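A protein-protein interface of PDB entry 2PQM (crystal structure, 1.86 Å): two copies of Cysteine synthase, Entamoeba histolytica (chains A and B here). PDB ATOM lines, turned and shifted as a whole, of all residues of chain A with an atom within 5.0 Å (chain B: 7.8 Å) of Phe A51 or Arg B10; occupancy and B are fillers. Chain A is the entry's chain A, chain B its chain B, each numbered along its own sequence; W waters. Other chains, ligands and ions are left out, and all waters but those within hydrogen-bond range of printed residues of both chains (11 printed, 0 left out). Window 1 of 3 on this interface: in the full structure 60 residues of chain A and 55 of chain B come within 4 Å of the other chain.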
ATOM      1  N   SER A   7     -22.868  12.100  21.744  1.00  0.00           N
ATOM      2  CA  SER A   7     -21.720  12.633  22.449  1.00  0.00           C
ATOM      3  C   SER A   7     -20.629  11.588  22.663  1.00  0.00           C
ATOM      4  O   SER A   7     -20.911  10.411  22.910  1.00  0.00           O
ATOM      5  CB  SER A   7     -22.156  13.229  23.795  1.00  0.00           C
ATOM      6  OG  SER A   7     -22.969  14.367  23.545  1.00  0.00           O
ATOM      7  N   ARG A  10     -16.535  11.544  28.011  1.00  0.00           N
ATOM      8  CA  ARG A  10     -15.944  12.695  28.704  1.00  0.00           C
ATOM      9  C   ARG A  10     -14.441  12.524  28.937  1.00  0.00           C
ATOM     10  O   ARG A  10     -13.736  13.521  29.075  1.00  0.00           O
ATOM     11  CB  ARG A  10     -16.676  12.933  30.025  1.00  0.00           C
ATOM     12  CG  ARG A  10     -18.104  13.498  29.805  1.00  0.00           C
ATOM     13  CD  ARG A  10     -18.995  13.246  30.990  1.00  0.00           C
ATOM     14  NE  ARG A  10     -20.286  13.939  30.812  1.00  0.00           N
ATOM     15  CZ  ARG A  10     -20.580  15.109  31.382  1.00  0.00           C
ATOM     16  NH1 ARG A  10     -19.689  15.696  32.168  1.00  0.00           N
ATOM     17  NH2 ARG A  10     -21.775  15.683  31.178  1.00  0.00           N
ATOM     18  N   THR A  20     -19.175  17.771  38.085  1.00  0.00           N
ATOM     19  CA  THR A  20     -19.976  17.636  36.849  1.00  0.00           C
ATOM     20  C   THR A  20     -20.812  18.883  36.556  1.00  0.00           C
ATOM     21  O   THR A  20     -21.566  18.922  35.573  1.00  0.00           O
ATOM     22  CB  THR A  20     -20.967  16.461  36.908  1.00  0.00           C
ATOM     23  OG1 THR A  20     -21.972  16.736  37.886  1.00  0.00           O
ATOM     24  CG2 THR A  20     -20.260  15.116  37.212  1.00  0.00           C
ATOM     25  N   GLY A  23     -20.021  23.309  31.981  1.00  0.00           N
ATOM     26  CA  GLY A  23     -19.721  22.734  30.663  1.00  0.00           C
ATOM     27  C   GLY A  23     -20.998  22.218  30.016  1.00  0.00           C
ATOM     28  O   GLY A  23     -21.043  21.095  29.509  1.00  0.00           O
ATOM     29  N   THR A  24     -22.049  23.036  30.060  1.00  0.00           N
ATOM     30  CA  THR A  24     -23.358  22.649  29.537  1.00  0.00           C
ATOM     31  C   THR A  24     -23.430  22.807  28.002  1.00  0.00           C
ATOM     32  O   THR A  24     -22.684  23.616  27.425  1.00  0.00           O
ATOM     33  CB  THR A  24     -24.478  23.515  30.185  1.00  0.00           C
ATOM     34  OG1 THR A  24     -24.171  24.886  29.966  1.00  0.00           O
ATOM     35  CG2 THR A  24     -24.555  23.257  31.679  1.00  0.00           C
ATOM     36  N   PRO A  25     -24.302  22.016  27.334  1.00  0.00           N
ATOM     37  CA  PRO A  25     -24.261  22.009  25.856  1.00  0.00           C
ATOM     38  C   PRO A  25     -24.984  23.172  25.175  1.00  0.00           C
ATOM     39  O   PRO A  25     -26.063  23.675  25.637  1.00  0.00           O
ATOM     40  CB  PRO A  25     -24.926  20.666  25.496  1.00  0.00           C
ATOM     41  CG  PRO A  25     -25.945  20.444  26.626  1.00  0.00           C
ATOM     42  CD  PRO A  25     -25.323  21.091  27.871  1.00  0.00           C
ATOM     43  N   LEU A  48     -28.127  24.743  27.465  1.00  0.00           N
ATOM     44  CA  LEU A  48     -29.086  23.962  28.244  1.00  0.00           C
ATOM     45  C   LEU A  48     -28.575  23.717  29.665  1.00  0.00           C
ATOM     46  O   LEU A  48     -27.846  22.738  29.946  1.00  0.00           O
ATOM     47  CB  LEU A  48     -29.399  22.630  27.509  1.00  0.00           C
ATOM     48  CG  LEU A  48     -29.891  22.780  26.065  1.00  0.00           C
ATOM     49  CD1 LEU A  48     -30.211  21.348  25.572  1.00  0.00           C
ATOM     50  CD2 LEU A  48     -31.142  23.694  25.904  1.00  0.00           C
ATOM     51  N   GLU A  49     -28.960  24.611  30.564  1.00  0.00           N
ATOM     52  CA  GLU A  49     -28.411  24.606  31.932  1.00  0.00           C
ATOM     53  C   GLU A  49     -29.010  23.505  32.786  1.00  0.00           C
ATOM     54  O   GLU A  49     -28.530  23.220  33.888  1.00  0.00           O
ATOM     55  CB  GLU A  49     -28.558  26.002  32.599  1.00  0.00           C
ATOM     56  CG  GLU A  49     -27.608  27.058  31.999  1.00  0.00           C
ATOM     57  CD  GLU A  49     -26.175  26.719  32.299  1.00  0.00           C
ATOM     58  OE1 GLU A  49     -25.889  26.399  33.464  1.00  0.00           O
ATOM     59  OE2 GLU A  49     -25.337  26.738  31.364  1.00  0.00           O
ATOM     60  N   TYR A  50     -30.048  22.851  32.263  1.00  0.00           N
ATOM     61  CA  TYR A  50     -30.567  21.659  32.936  1.00  0.00           C
ATOM     62  C   TYR A  50     -29.677  20.402  32.799  1.00  0.00           C
ATOM     63  O   TYR A  50     -29.954  19.382  33.423  1.00  0.00           O
ATOM     64  CB  TYR A  50     -32.019  21.392  32.555  1.00  0.00           C
ATOM     65  CG  TYR A  50     -32.325  21.124  31.089  1.00  0.00           C
ATOM     66  CD1 TYR A  50     -32.115  19.872  30.534  1.00  0.00           C
ATOM     67  CD2 TYR A  50     -32.878  22.129  30.280  1.00  0.00           C
ATOM     68  CE1 TYR A  50     -32.463  19.605  29.218  1.00  0.00           C
ATOM     69  CE2 TYR A  50     -33.227  21.884  28.956  1.00  0.00           C
ATOM     70  CZ  TYR A  50     -33.015  20.606  28.443  1.00  0.00           C
ATOM     71  OH  TYR A  50     -33.355  20.333  27.168  1.00  0.00           O
ATOM     72  N   PHE A  51     -28.600  20.481  31.999  1.00  0.00           N
ATOM     73  CA  PHE A  51     -27.570  19.434  31.998  1.00  0.00           C
ATOM     74  C   PHE A  51     -26.740  19.396  33.276  1.00  0.00           C
ATOM     75  O   PHE A  51     -26.051  18.430  33.529  1.00  0.00           O
ATOM     76  CB  PHE A  51     -26.687  19.538  30.753  1.00  0.00           C
ATOM     77  CG  PHE A  51     -27.301  18.835  29.564  1.00  0.00           C
ATOM     78  CD1 PHE A  51     -28.484  19.337  28.988  1.00  0.00           C
ATOM     79  CD2 PHE A  51     -26.719  17.671  29.046  1.00  0.00           C
ATOM     80  CE1 PHE A  51     -29.083  18.682  27.890  1.00  0.00           C
ATOM     81  CE2 PHE A  51     -27.301  17.022  27.965  1.00  0.00           C
ATOM     82  CZ  PHE A  51     -28.482  17.526  27.399  1.00  0.00           C
ATOM     83  N   ASN A  52     -26.815  20.448  34.085  1.00  0.00           N
ATOM     84  CA  ASN A  52     -26.226  20.410  35.457  1.00  0.00           C
ATOM     85  C   ASN A  52     -26.804  19.243  36.283  1.00  0.00           C
ATOM     86  O   ASN A  52     -27.905  18.768  35.986  1.00  0.00           O
ATOM     87  CB  ASN A  52     -26.484  21.750  36.158  1.00  0.00           C
ATOM     88  CG  ASN A  52     -25.575  22.848  35.664  1.00  0.00           C
ATOM     89  OD1 ASN A  52     -26.023  23.880  35.133  1.00  0.00           O
ATOM     90  ND2 ASN A  52     -24.282  22.664  35.890  1.00  0.00           N
ATOM     91  N   PRO A  53     -26.041  18.730  37.286  1.00  0.00           N
ATOM     92  CA  PRO A  53     -26.506  17.497  37.984  1.00  0.00           C
ATOM     93  C   PRO A  53     -27.895  17.542  38.651  1.00  0.00           C
ATOM     94  O   PRO A  53     -28.580  16.524  38.703  1.00  0.00           O
ATOM     95  CB  PRO A  53     -25.420  17.232  39.020  1.00  0.00           C
ATOM     96  CG  PRO A  53     -24.579  18.547  39.121  1.00  0.00           C
ATOM     97  CD  PRO A  53     -24.678  19.137  37.716  1.00  0.00           C
ATOM     98  N   ASP A 179     -17.345  27.506  22.918  1.00  0.00           N
ATOM     99  CA  ASP A 179     -18.235  26.671  22.091  1.00  0.00           C
ATOM    100  C   ASP A 179     -18.577  27.313  20.753  1.00  0.00           C
ATOM    101  O   ASP A 179     -18.770  26.591  19.764  1.00  0.00           O
ATOM    102  CB  ASP A 179     -19.508  26.266  22.824  1.00  0.00           C
ATOM    103  CG  ASP A 179     -19.245  25.298  23.977  1.00  0.00           C
ATOM    104  OD1 ASP A 179     -18.105  24.769  24.112  1.00  0.00           O
ATOM    105  OD2 ASP A 179     -20.193  25.059  24.748  1.00  0.00           O
ATOM    106  N   SER B   7     -16.757  21.457  35.364  1.00  0.00           N
ATOM    107  CA  SER B   7     -16.500  20.945  34.004  1.00  0.00           C
ATOM    108  C   SER B   7     -16.056  22.029  33.035  1.00  0.00           C
ATOM    109  O   SER B   7     -16.461  23.194  33.139  1.00  0.00           O
ATOM    110  CB  SER B   7     -17.696  20.181  33.436  1.00  0.00           C
ATOM    111  OG  SER B   7     -17.981  19.052  34.251  1.00  0.00           O
ATOM    112  N   SER B   8     -15.216  21.631  32.086  1.00  0.00           N
ATOM    113  CA  SER B   8     -14.695  22.538  31.072  1.00  0.00           C
ATOM    114  C   SER B   8     -15.692  22.607  29.911  1.00  0.00           C
ATOM    115  O   SER B   8     -16.591  21.749  29.814  1.00  0.00           O
ATOM    116  CB  SER B   8     -13.344  22.013  30.552  1.00  0.00           C
ATOM    117  OG  SER B   8     -12.376  22.112  31.586  1.00  0.00           O
ATOM    118  N   PRO B   9     -15.545  23.622  29.052  1.00  0.00           N
ATOM    119  CA  PRO B   9     -16.408  23.722  27.872  1.00  0.00           C
ATOM    120  C   PRO B   9     -16.377  22.457  27.026  1.00  0.00           C
ATOM    121  O   PRO B   9     -15.329  21.810  26.888  1.00  0.00           O
ATOM    122  CB  PRO B   9     -15.814  24.909  27.091  1.00  0.00           C
ATOM    123  CG  PRO B   9     -15.188  25.778  28.154  1.00  0.00           C
ATOM    124  CD  PRO B   9     -14.611  24.772  29.145  1.00  0.00           C
ATOM    125  N   ARG B  10     -17.529  22.103  26.463  1.00  0.00           N
ATOM    126  CA  ARG B  10     -17.633  20.941  25.579  1.00  0.00           C
ATOM    127  C   ARG B  10     -16.913  21.143  24.241  1.00  0.00           C
ATOM    128  O   ARG B  10     -16.538  20.167  23.618  1.00  0.00           O
ATOM    129  CB  ARG B  10     -19.112  20.593  25.309  1.00  0.00           C
ATOM    130  CG  ARG B  10     -19.805  19.910  26.518  1.00  0.00           C
ATOM    131  CD  ARG B  10     -21.325  20.049  26.438  1.00  0.00           C
ATOM    132  NE  ARG B  10     -21.979  19.345  27.553  1.00  0.00           N
ATOM    133  CZ  ARG B  10     -22.551  18.147  27.464  1.00  0.00           C
ATOM    134  NH1 ARG B  10     -22.556  17.501  26.302  1.00  0.00           N
ATOM    135  NH2 ARG B  10     -23.127  17.590  28.550  1.00  0.00           N
ATOM    136  N   LYS B  11     -16.722  22.399  23.837  1.00  0.00           N
ATOM    137  CA  LYS B  11     -16.140  22.776  22.535  1.00  0.00           C
ATOM    138  C   LYS B  11     -16.854  22.063  21.372  1.00  0.00           C
ATOM    139  O   LYS B  11     -16.214  21.418  20.526  1.00  0.00           O
ATOM    140  CB  LYS B  11     -14.610  22.527  22.497  1.00  0.00           C
ATOM    141  CG  LYS B  11     -13.831  23.201  23.644  1.00  0.00           C
ATOM    142  CD  LYS B  11     -12.300  22.996  23.601  1.00  0.00           C
ATOM    143  CE  LYS B  11     -11.924  21.497  23.598  1.00  0.00           C
ATOM    144  NZ  LYS B  11     -10.443  21.211  23.848  1.00  0.00           N
ATOM    145  N   ARG B  12     -18.177  22.158  21.360  1.00  0.00           N
ATOM    146  CA  ARG B  12     -19.029  21.548  20.327  1.00  0.00           C
ATOM    147  C   ARG B  12     -20.278  22.411  20.270  1.00  0.00           C
ATOM    148  O   ARG B  12     -20.690  22.958  21.316  1.00  0.00           O
ATOM    149  CB  ARG B  12     -19.385  20.056  20.634  1.00  0.00           C
ATOM    150  CG  ARG B  12     -20.118  19.307  19.424  1.00  0.00           C
ATOM    151  CD  ARG B  12     -20.205  17.763  19.492  1.00  0.00           C
ATOM    152  NE  ARG B  12     -21.095  17.231  18.446  1.00  0.00           N
ATOM    153  CZ  ARG B  12     -21.685  16.035  18.444  1.00  0.00           C
ATOM    154  NH1 ARG B  12     -21.552  15.163  19.457  1.00  0.00           N
ATOM    155  NH2 ARG B  12     -22.451  15.707  17.415  1.00  0.00           N
ATOM    156  N   ILE B  13     -20.818  22.615  19.064  1.00  0.00           N
ATOM    157  CA  ILE B  13     -22.214  23.055  18.913  1.00  0.00           C
ATOM    158  C   ILE B  13     -23.000  21.862  18.370  1.00  0.00           C
ATOM    159  O   ILE B  13     -22.700  21.335  17.289  1.00  0.00           O
ATOM    160  CB  ILE B  13     -22.349  24.301  18.006  1.00  0.00           C
ATOM    161  CG1 ILE B  13     -21.821  25.540  18.734  1.00  0.00           C
ATOM    162  CG2 ILE B  13     -23.807  24.512  17.579  1.00  0.00           C
ATOM    163  CD1 ILE B  13     -21.618  26.763  17.829  1.00  0.00           C
ATOM    164  N   TYR B  14     -23.996  21.429  19.140  1.00  0.00           N
ATOM    165  CA  TYR B  14     -24.805  20.266  18.829  1.00  0.00           C
ATOM    166  C   TYR B  14     -25.876  20.681  17.817  1.00  0.00           C
ATOM    167  O   TYR B  14     -26.504  21.750  17.955  1.00  0.00           O
ATOM    168  CB  TYR B  14     -25.434  19.718  20.125  1.00  0.00           C
ATOM    169  CG  TYR B  14     -24.362  19.306  21.093  1.00  0.00           C
ATOM    170  CD1 TYR B  14     -23.867  18.004  21.088  1.00  0.00           C
ATOM    171  CD2 TYR B  14     -23.782  20.229  21.971  1.00  0.00           C
ATOM    172  CE1 TYR B  14     -22.861  17.629  21.957  1.00  0.00           C
ATOM    173  CE2 TYR B  14     -22.759  19.868  22.817  1.00  0.00           C
ATOM    174  CZ  TYR B  14     -22.299  18.560  22.804  1.00  0.00           C
ATOM    175  OH  TYR B  14     -21.287  18.160  23.649  1.00  0.00           O
ATOM    176  N   ILE B  17     -30.889  18.038  19.807  1.00  0.00           N
ATOM    177  CA  ILE B  17     -30.819  17.543  21.190  1.00  0.00           C
ATOM    178  C   ILE B  17     -30.327  16.084  21.252  1.00  0.00           C
ATOM    179  O   ILE B  17     -29.804  15.639  22.270  1.00  0.00           O
ATOM    180  CB  ILE B  17     -32.219  17.719  21.926  1.00  0.00           C
ATOM    181  CG1 ILE B  17     -32.106  17.459  23.432  1.00  0.00           C
ATOM    182  CG2 ILE B  17     -33.320  16.872  21.302  1.00  0.00           C
ATOM    183  CD1 ILE B  17     -31.312  18.512  24.172  1.00  0.00           C
ATOM    184  N   GLU B  19     -27.963  14.778  19.653  1.00  0.00           N
ATOM    185  CA  GLU B  19     -26.507  14.779  19.684  1.00  0.00           C
ATOM    186  C   GLU B  19     -25.923  14.945  21.094  1.00  0.00           C
ATOM    187  O   GLU B  19     -24.723  14.722  21.302  1.00  0.00           O
ATOM    188  CB  GLU B  19     -25.936  15.839  18.715  1.00  0.00           C
ATOM    189  CG  GLU B  19     -26.267  15.512  17.253  1.00  0.00           C
ATOM    190  CD  GLU B  19     -25.343  16.221  16.279  1.00  0.00           C
ATOM    191  OE1 GLU B  19     -24.956  17.377  16.547  1.00  0.00           O
ATOM    192  OE2 GLU B  19     -24.977  15.576  15.268  1.00  0.00           O
ATOM    193  N   THR B  20     -26.776  15.341  22.043  1.00  0.00           N
ATOM    194  CA  THR B  20     -26.363  15.487  23.444  1.00  0.00           C
ATOM    195  C   THR B  20     -26.575  14.211  24.229  1.00  0.00           C
ATOM    196  O   THR B  20     -26.222  14.146  25.404  1.00  0.00           O
ATOM    197  CB  THR B  20     -27.104  16.641  24.181  1.00  0.00           C
ATOM    198  OG1 THR B  20     -28.480  16.284  24.379  1.00  0.00           O
ATOM    199  CG2 THR B  20     -26.989  17.981  23.376  1.00  0.00           C
ATOM    200  N   ILE B  21     -27.145  13.194  23.585  1.00  0.00           N
ATOM    201  CA  ILE B  21     -27.346  11.890  24.233  1.00  0.00           C
ATOM    202  C   ILE B  21     -25.987  11.233  24.450  1.00  0.00           C
ATOM    203  O   ILE B  21     -25.095  11.398  23.635  1.00  0.00           O
ATOM    204  CB  ILE B  21     -28.299  10.997  23.396  1.00  0.00           C
ATOM    205  CG1 ILE B  21     -29.731  11.598  23.402  1.00  0.00           C
ATOM    206  CG2 ILE B  21     -28.259   9.508  23.895  1.00  0.00           C
ATOM    207  CD1 ILE B  21     -30.716  10.968  22.384  1.00  0.00           C
ATOM    208  N   GLY B  22     -25.825  10.499  25.540  1.00  0.00           N
ATOM    209  CA  GLY B  22     -24.584   9.726  25.762  1.00  0.00           C
ATOM    210  C   GLY B  22     -23.447  10.585  26.327  1.00  0.00           C
ATOM    211  O   GLY B  22     -23.659  11.745  26.748  1.00  0.00           O
ATOM    212  N   GLY B  23     -22.237  10.027  26.316  1.00  0.00           N
ATOM    213  CA  GLY B  23     -21.080  10.656  26.970  1.00  0.00           C
ATOM    214  C   GLY B  23     -21.420  11.087  28.401  1.00  0.00           C
ATOM    215  O   GLY B  23     -21.108  12.210  28.796  1.00  0.00           O
ATOM    216  N   THR B  24     -22.053  10.192  29.158  1.00  0.00           N
ATOM    217  CA  THR B  24     -22.541  10.495  30.524  1.00  0.00           C
ATOM    218  C   THR B  24     -21.378  10.386  31.534  1.00  0.00           C
ATOM    219  O   THR B  24     -20.420   9.641  31.303  1.00  0.00           O
ATOM    220  CB  THR B  24     -23.718   9.584  30.943  1.00  0.00           C
ATOM    221  OG1 THR B  24     -23.291   8.216  30.876  1.00  0.00           O
ATOM    222  CG2 THR B  24     -24.982   9.771  30.008  1.00  0.00           C
ATOM    223  N   PRO B  25     -21.434  11.154  32.639  1.00  0.00           N
ATOM    224  CA  PRO B  25     -20.286  11.212  33.562  1.00  0.00           C
ATOM    225  C   PRO B  25     -20.137   9.998  34.475  1.00  0.00           C
ATOM    226  O   PRO B  25     -21.120   9.395  34.930  1.00  0.00           O
ATOM    227  CB  PRO B  25     -20.543  12.485  34.389  1.00  0.00           C
ATOM    228  CG  PRO B  25     -22.089  12.619  34.417  1.00  0.00           C
ATOM    229  CD  PRO B  25     -22.546  12.033  33.059  1.00  0.00           C
ATOM    230  N   TYR B  50     -28.797   9.802  33.945  1.00  0.00           N
ATOM    231  CA  TYR B  50     -29.767  10.901  33.998  1.00  0.00           C
ATOM    232  C   TYR B  50     -29.182  12.214  33.489  1.00  0.00           C
ATOM    233  O   TYR B  50     -29.893  13.215  33.386  1.00  0.00           O
ATOM    234  CB  TYR B  50     -30.381  11.051  35.402  1.00  0.00           C
ATOM    235  CG  TYR B  50     -29.447  11.376  36.531  1.00  0.00           C
ATOM    236  CD1 TYR B  50     -28.934  12.664  36.717  1.00  0.00           C
ATOM    237  CD2 TYR B  50     -29.167  10.410  37.502  1.00  0.00           C
ATOM    238  CE1 TYR B  50     -28.076  12.949  37.817  1.00  0.00           C
ATOM    239  CE2 TYR B  50     -28.363  10.680  38.570  1.00  0.00           C
ATOM    240  CZ  TYR B  50     -27.829  11.940  38.743  1.00  0.00           C
ATOM    241  OH  TYR B  50     -27.063  12.163  39.859  1.00  0.00           O
ATOM    242  N   PHE B  51     -27.901  12.207  33.124  1.00  0.00           N
ATOM    243  CA  PHE B  51     -27.340  13.332  32.389  1.00  0.00           C
ATOM    244  C   PHE B  51     -27.821  13.413  30.924  1.00  0.00           C
ATOM    245  O   PHE B  51     -27.624  14.425  30.277  1.00  0.00           O
ATOM    246  CB  PHE B  51     -25.821  13.335  32.448  1.00  0.00           C
ATOM    247  CG  PHE B  51     -25.267  14.015  33.673  1.00  0.00           C
ATOM    248  CD1 PHE B  51     -25.479  13.471  34.947  1.00  0.00           C
ATOM    249  CD2 PHE B  51     -24.571  15.225  33.543  1.00  0.00           C
ATOM    250  CE1 PHE B  51     -24.963  14.107  36.087  1.00  0.00           C
ATOM    251  CE2 PHE B  51     -24.035  15.880  34.665  1.00  0.00           C
ATOM    252  CZ  PHE B  51     -24.232  15.317  35.933  1.00  0.00           C
ATOM    253  N   ASN B  52     -28.397  12.334  30.397  1.00  0.00           N
ATOM    254  CA  ASN B  52     -29.075  12.381  29.086  1.00  0.00           C
ATOM    255  C   ASN B  52     -30.147  13.479  29.045  1.00  0.00           C
ATOM    256  O   ASN B  52     -30.658  13.867  30.089  1.00  0.00           O
ATOM    257  CB  ASN B  52     -29.702  11.025  28.757  1.00  0.00           C
ATOM    258  CG  ASN B  52     -28.663   9.989  28.353  1.00  0.00           C
ATOM    259  OD1 ASN B  52     -28.461   8.971  29.040  1.00  0.00           O
ATOM    260  ND2 ASN B  52     -27.971  10.264  27.263  1.00  0.00           N
ATOM    261  N   PRO B  53     -30.472  14.001  27.845  1.00  0.00           N
ATOM    262  CA  PRO B  53     -31.383  15.162  27.816  1.00  0.00           C
ATOM    263  C   PRO B  53     -32.739  14.969  28.471  1.00  0.00           C
ATOM    264  O   PRO B  53     -33.263  15.946  29.004  1.00  0.00           O
ATOM    265  CB  PRO B  53     -31.505  15.498  26.318  1.00  0.00           C
ATOM    266  CG  PRO B  53     -31.010  14.281  25.625  1.00  0.00           C
ATOM    267  CD  PRO B  53     -29.941  13.712  26.505  1.00  0.00           C
ATOM    268  N   MET B  54     -33.332  13.771  28.419  1.00  0.00           N
ATOM    269  CA  MET B  54     -34.565  13.529  29.189  1.00  0.00           C
ATOM    270  C   MET B  54     -34.351  12.703  30.468  1.00  0.00           C
ATOM    271  O   MET B  54     -35.292  12.090  31.009  1.00  0.00           O
ATOM    272  CB  MET B  54     -35.705  12.969  28.307  1.00  0.00           C
ATOM    273  CG  MET B  54     -36.360  14.076  27.409  1.00  0.00           C
ATOM    274  SD  MET B  54     -37.013  15.428  28.430  1.00  0.00           S
ATOM    275  CE  MET B  54     -38.187  14.552  29.454  1.00  0.00           C
ATOM    276  N   SER B  55     -33.117  12.727  30.964  1.00  0.00           N
ATOM    277  CA  SER B  55     -32.787  12.257  32.320  1.00  0.00           C
ATOM    278  C   SER B  55     -32.944  10.752  32.530  1.00  0.00           C
ATOM    279  O   SER B  55     -33.212  10.311  33.637  1.00  0.00           O
ATOM    280  CB  SER B  55     -33.537  13.061  33.433  1.00  0.00           C
ATOM    281  OG  SER B  55     -33.051  14.396  33.498  1.00  0.00           O
ATOM    282  N   ASP B  59     -33.030   7.360  26.827  1.00  0.00           N
ATOM    283  CA  ASP B  59     -32.729   8.308  25.750  1.00  0.00           C
ATOM    284  C   ASP B  59     -31.889   7.641  24.651  1.00  0.00           C
ATOM    285  O   ASP B  59     -32.175   7.816  23.460  1.00  0.00           O
ATOM    286  CB  ASP B  59     -31.979   9.524  26.280  1.00  0.00           C
ATOM    287  CG  ASP B  59     -32.880  10.473  27.002  1.00  0.00           C
ATOM    288  OD1 ASP B  59     -33.948  10.035  27.435  1.00  0.00           O
ATOM    289  OD2 ASP B  59     -32.538  11.657  27.080  1.00  0.00           O
ATOM    290  N   GLN B  95     -39.133  12.030  22.424  1.00  0.00           N
ATOM    291  CA  GLN B  95     -38.027  12.934  22.103  1.00  0.00           C
ATOM    292  C   GLN B  95     -37.480  12.690  20.689  1.00  0.00           C
ATOM    293  O   GLN B  95     -37.323  13.628  19.890  1.00  0.00           O
ATOM    294  CB  GLN B  95     -36.921  12.786  23.170  1.00  0.00           C
ATOM    295  CG  GLN B  95     -35.640  13.599  22.919  1.00  0.00           C
ATOM    296  CD  GLN B  95     -34.603  13.341  24.039  1.00  0.00           C
ATOM    297  OE1 GLN B  95     -34.120  12.212  24.247  1.00  0.00           O
ATOM    298  NE2 GLN B  95     -34.279  14.360  24.742  1.00  0.00           N
HETATM  299  O   HOH W   1     -18.391   9.640  29.311  1.00  0.00           O
HETATM  300  O   HOH W   2     -23.466  18.012  31.424  1.00  0.00           O
HETATM  301  O   HOH W   3     -27.898  14.393  40.897  1.00  0.00           O
HETATM  302  O   HOH W   4     -19.838  23.809  27.147  1.00  0.00           O
HETATM  303  O   HOH W   5     -20.503  18.304  33.198  1.00  0.00           O
HETATM  304  O   HOH W   6     -30.842  16.074  33.405  1.00  0.00           O
HETATM  305  O   HOH W   7     -34.640  18.055  26.983  1.00  0.00           O
HETATM  306  O   HOH W   8     -23.785  15.075  26.071  1.00  0.00           O
HETATM  307  O   HOH W   9     -21.685  22.853  23.795  1.00  0.00           O
HETATM  308  O   HOH W  10     -24.069  14.899  29.454  1.00  0.00           O
HETATM  309  O   HOH W  11     -17.192  24.346  19.166  1.00  0.00           O
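The backbone NH (N) of Ser A7 lies within hydrogen-bond range of the backbone carbonyl oxygen (O) of Ile B21, at 3.0 Å. O of Gly B23 sits at hydrogen-bond distance from NE of Arg A10 (2.8 Å). NE of Arg B10 lies within hydrogen-bond range of O of Gly A23 (2.8 Å). The side-chain hydroxyl of Ser A7 lies within hydrogen-bond range of the backbone carbonyl oxygen of Glu B19, at 2.9 Å. OD1 of Asp A179 lies within hydrogen-bond range of N of Lys B11 (2.8 Å).
The guanidinium group (NH1) of Arg B10 lies within hydrogen-bond range of the side-chain hydroxyl (OH) of Tyr B14 (3.0 Å). The backbone carbonyl oxygen (O) of Tyr B50 sits close to the side-chain hydroxyl (OG) of Ser B55 (3.4 Å). The backbone carbonyl oxygen (O) of Ile B17 lies within hydrogen-bond range of the side-chain hydroxyl (OG1) of Thr B20, at 2.6 Å. OE2 of Glu A49 lies within hydrogen-bond range of OG1 of Thr A24 (2.6 Å).
Ser A7 touches Thr B20. Gly B23 touches Ser A7. NH2 of Arg B10 touches NH2 of Arg A10 (3.5 Å). Arg A10 touches Pro B25. Thr A20 touches Ser B7 (CA to OG, 3.6 Å). Phe B51 touches Thr A20. NE of Arg B10 touches N of Pro A25, 3.5 Å away. Ile B17 touches Leu A48. Phe A51 touches Thr B20. Arg B12 touches Asp A179 (N to OD1, 3.8 Å).
Printed residues of chain B within 4 Å of Pro A25: Arg B10 (3.5 Å), Tyr B14 (3.5 Å) and Thr B20 (3.99 Å). Of chain B, only Arg B10 (3.6 Å), Thr B20 (3.3 Å), Phe B51 (3.4 Å) and Pro B53 (3.8 Å) come within 4 Å of Phe A51. Of chain A, only Arg A10 (3.5 Å), Gly A23 (2.8 Å), Thr A24 (3.8 Å), Pro A25 (3.5 Å), Phe A51 (3.6 Å) and Asp A179 (3.6 Å) come within 4 Å of Arg B10. Of the printed residues of chain A, Arg B12 touches Ser A7 and Asp A179. Of the printed residues of chain A, Ile B17 touches Leu A48. Of the printed residues of chain A, Ile B21 touches Ser A7 (3.0 Å). Of the printed residues of chain A, Thr B24 touches Arg A10 (3.8 Å). Asp B59 touches none of the printed residues of chain A.
Hydrophobic or aromatic side chains of chain A that line the printed part of chain B: Pro A25, Leu A48, Tyr A50, Phe A51 and Pro A53. Of the 24 printed residues of chain B, 19 touch a printed residue of chain A. Hydrophobic or aromatic side chains of chain B that line the printed part of chain A: Pro B9, Ile B13, Tyr B14, Ile B17, Pro B25, Tyr B50, Phe B51 and Pro B53. Among the printed residues, 35 pairs touch across the chains.
Arg A10 touches Gly B23, and with the chains exchanged Gly A23 touches Arg B10. Arg A10 touches Phe B51, and with the chains exchanged Phe A51 touches Arg B10. Phe A51 touches Pro B53, and with the chains exchanged Pro A53 touches Phe B51. Of the 35 pairs that touch across the chains among the printed residues, 22 have their exchanged pair printed and touching as well.
Water W7 bridges the side-chain hydroxyl of Tyr A50 (2.6 Å) and the backbone carbonyl oxygen of Pro B53 (3.2 Å). Water W1 bridges O of Thr B24 (2.8 Å) and N of Arg A10 (3.0 Å). Water W10 bridges the guanidinium group of Arg A10 and the guanidinium group of Arg B10.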
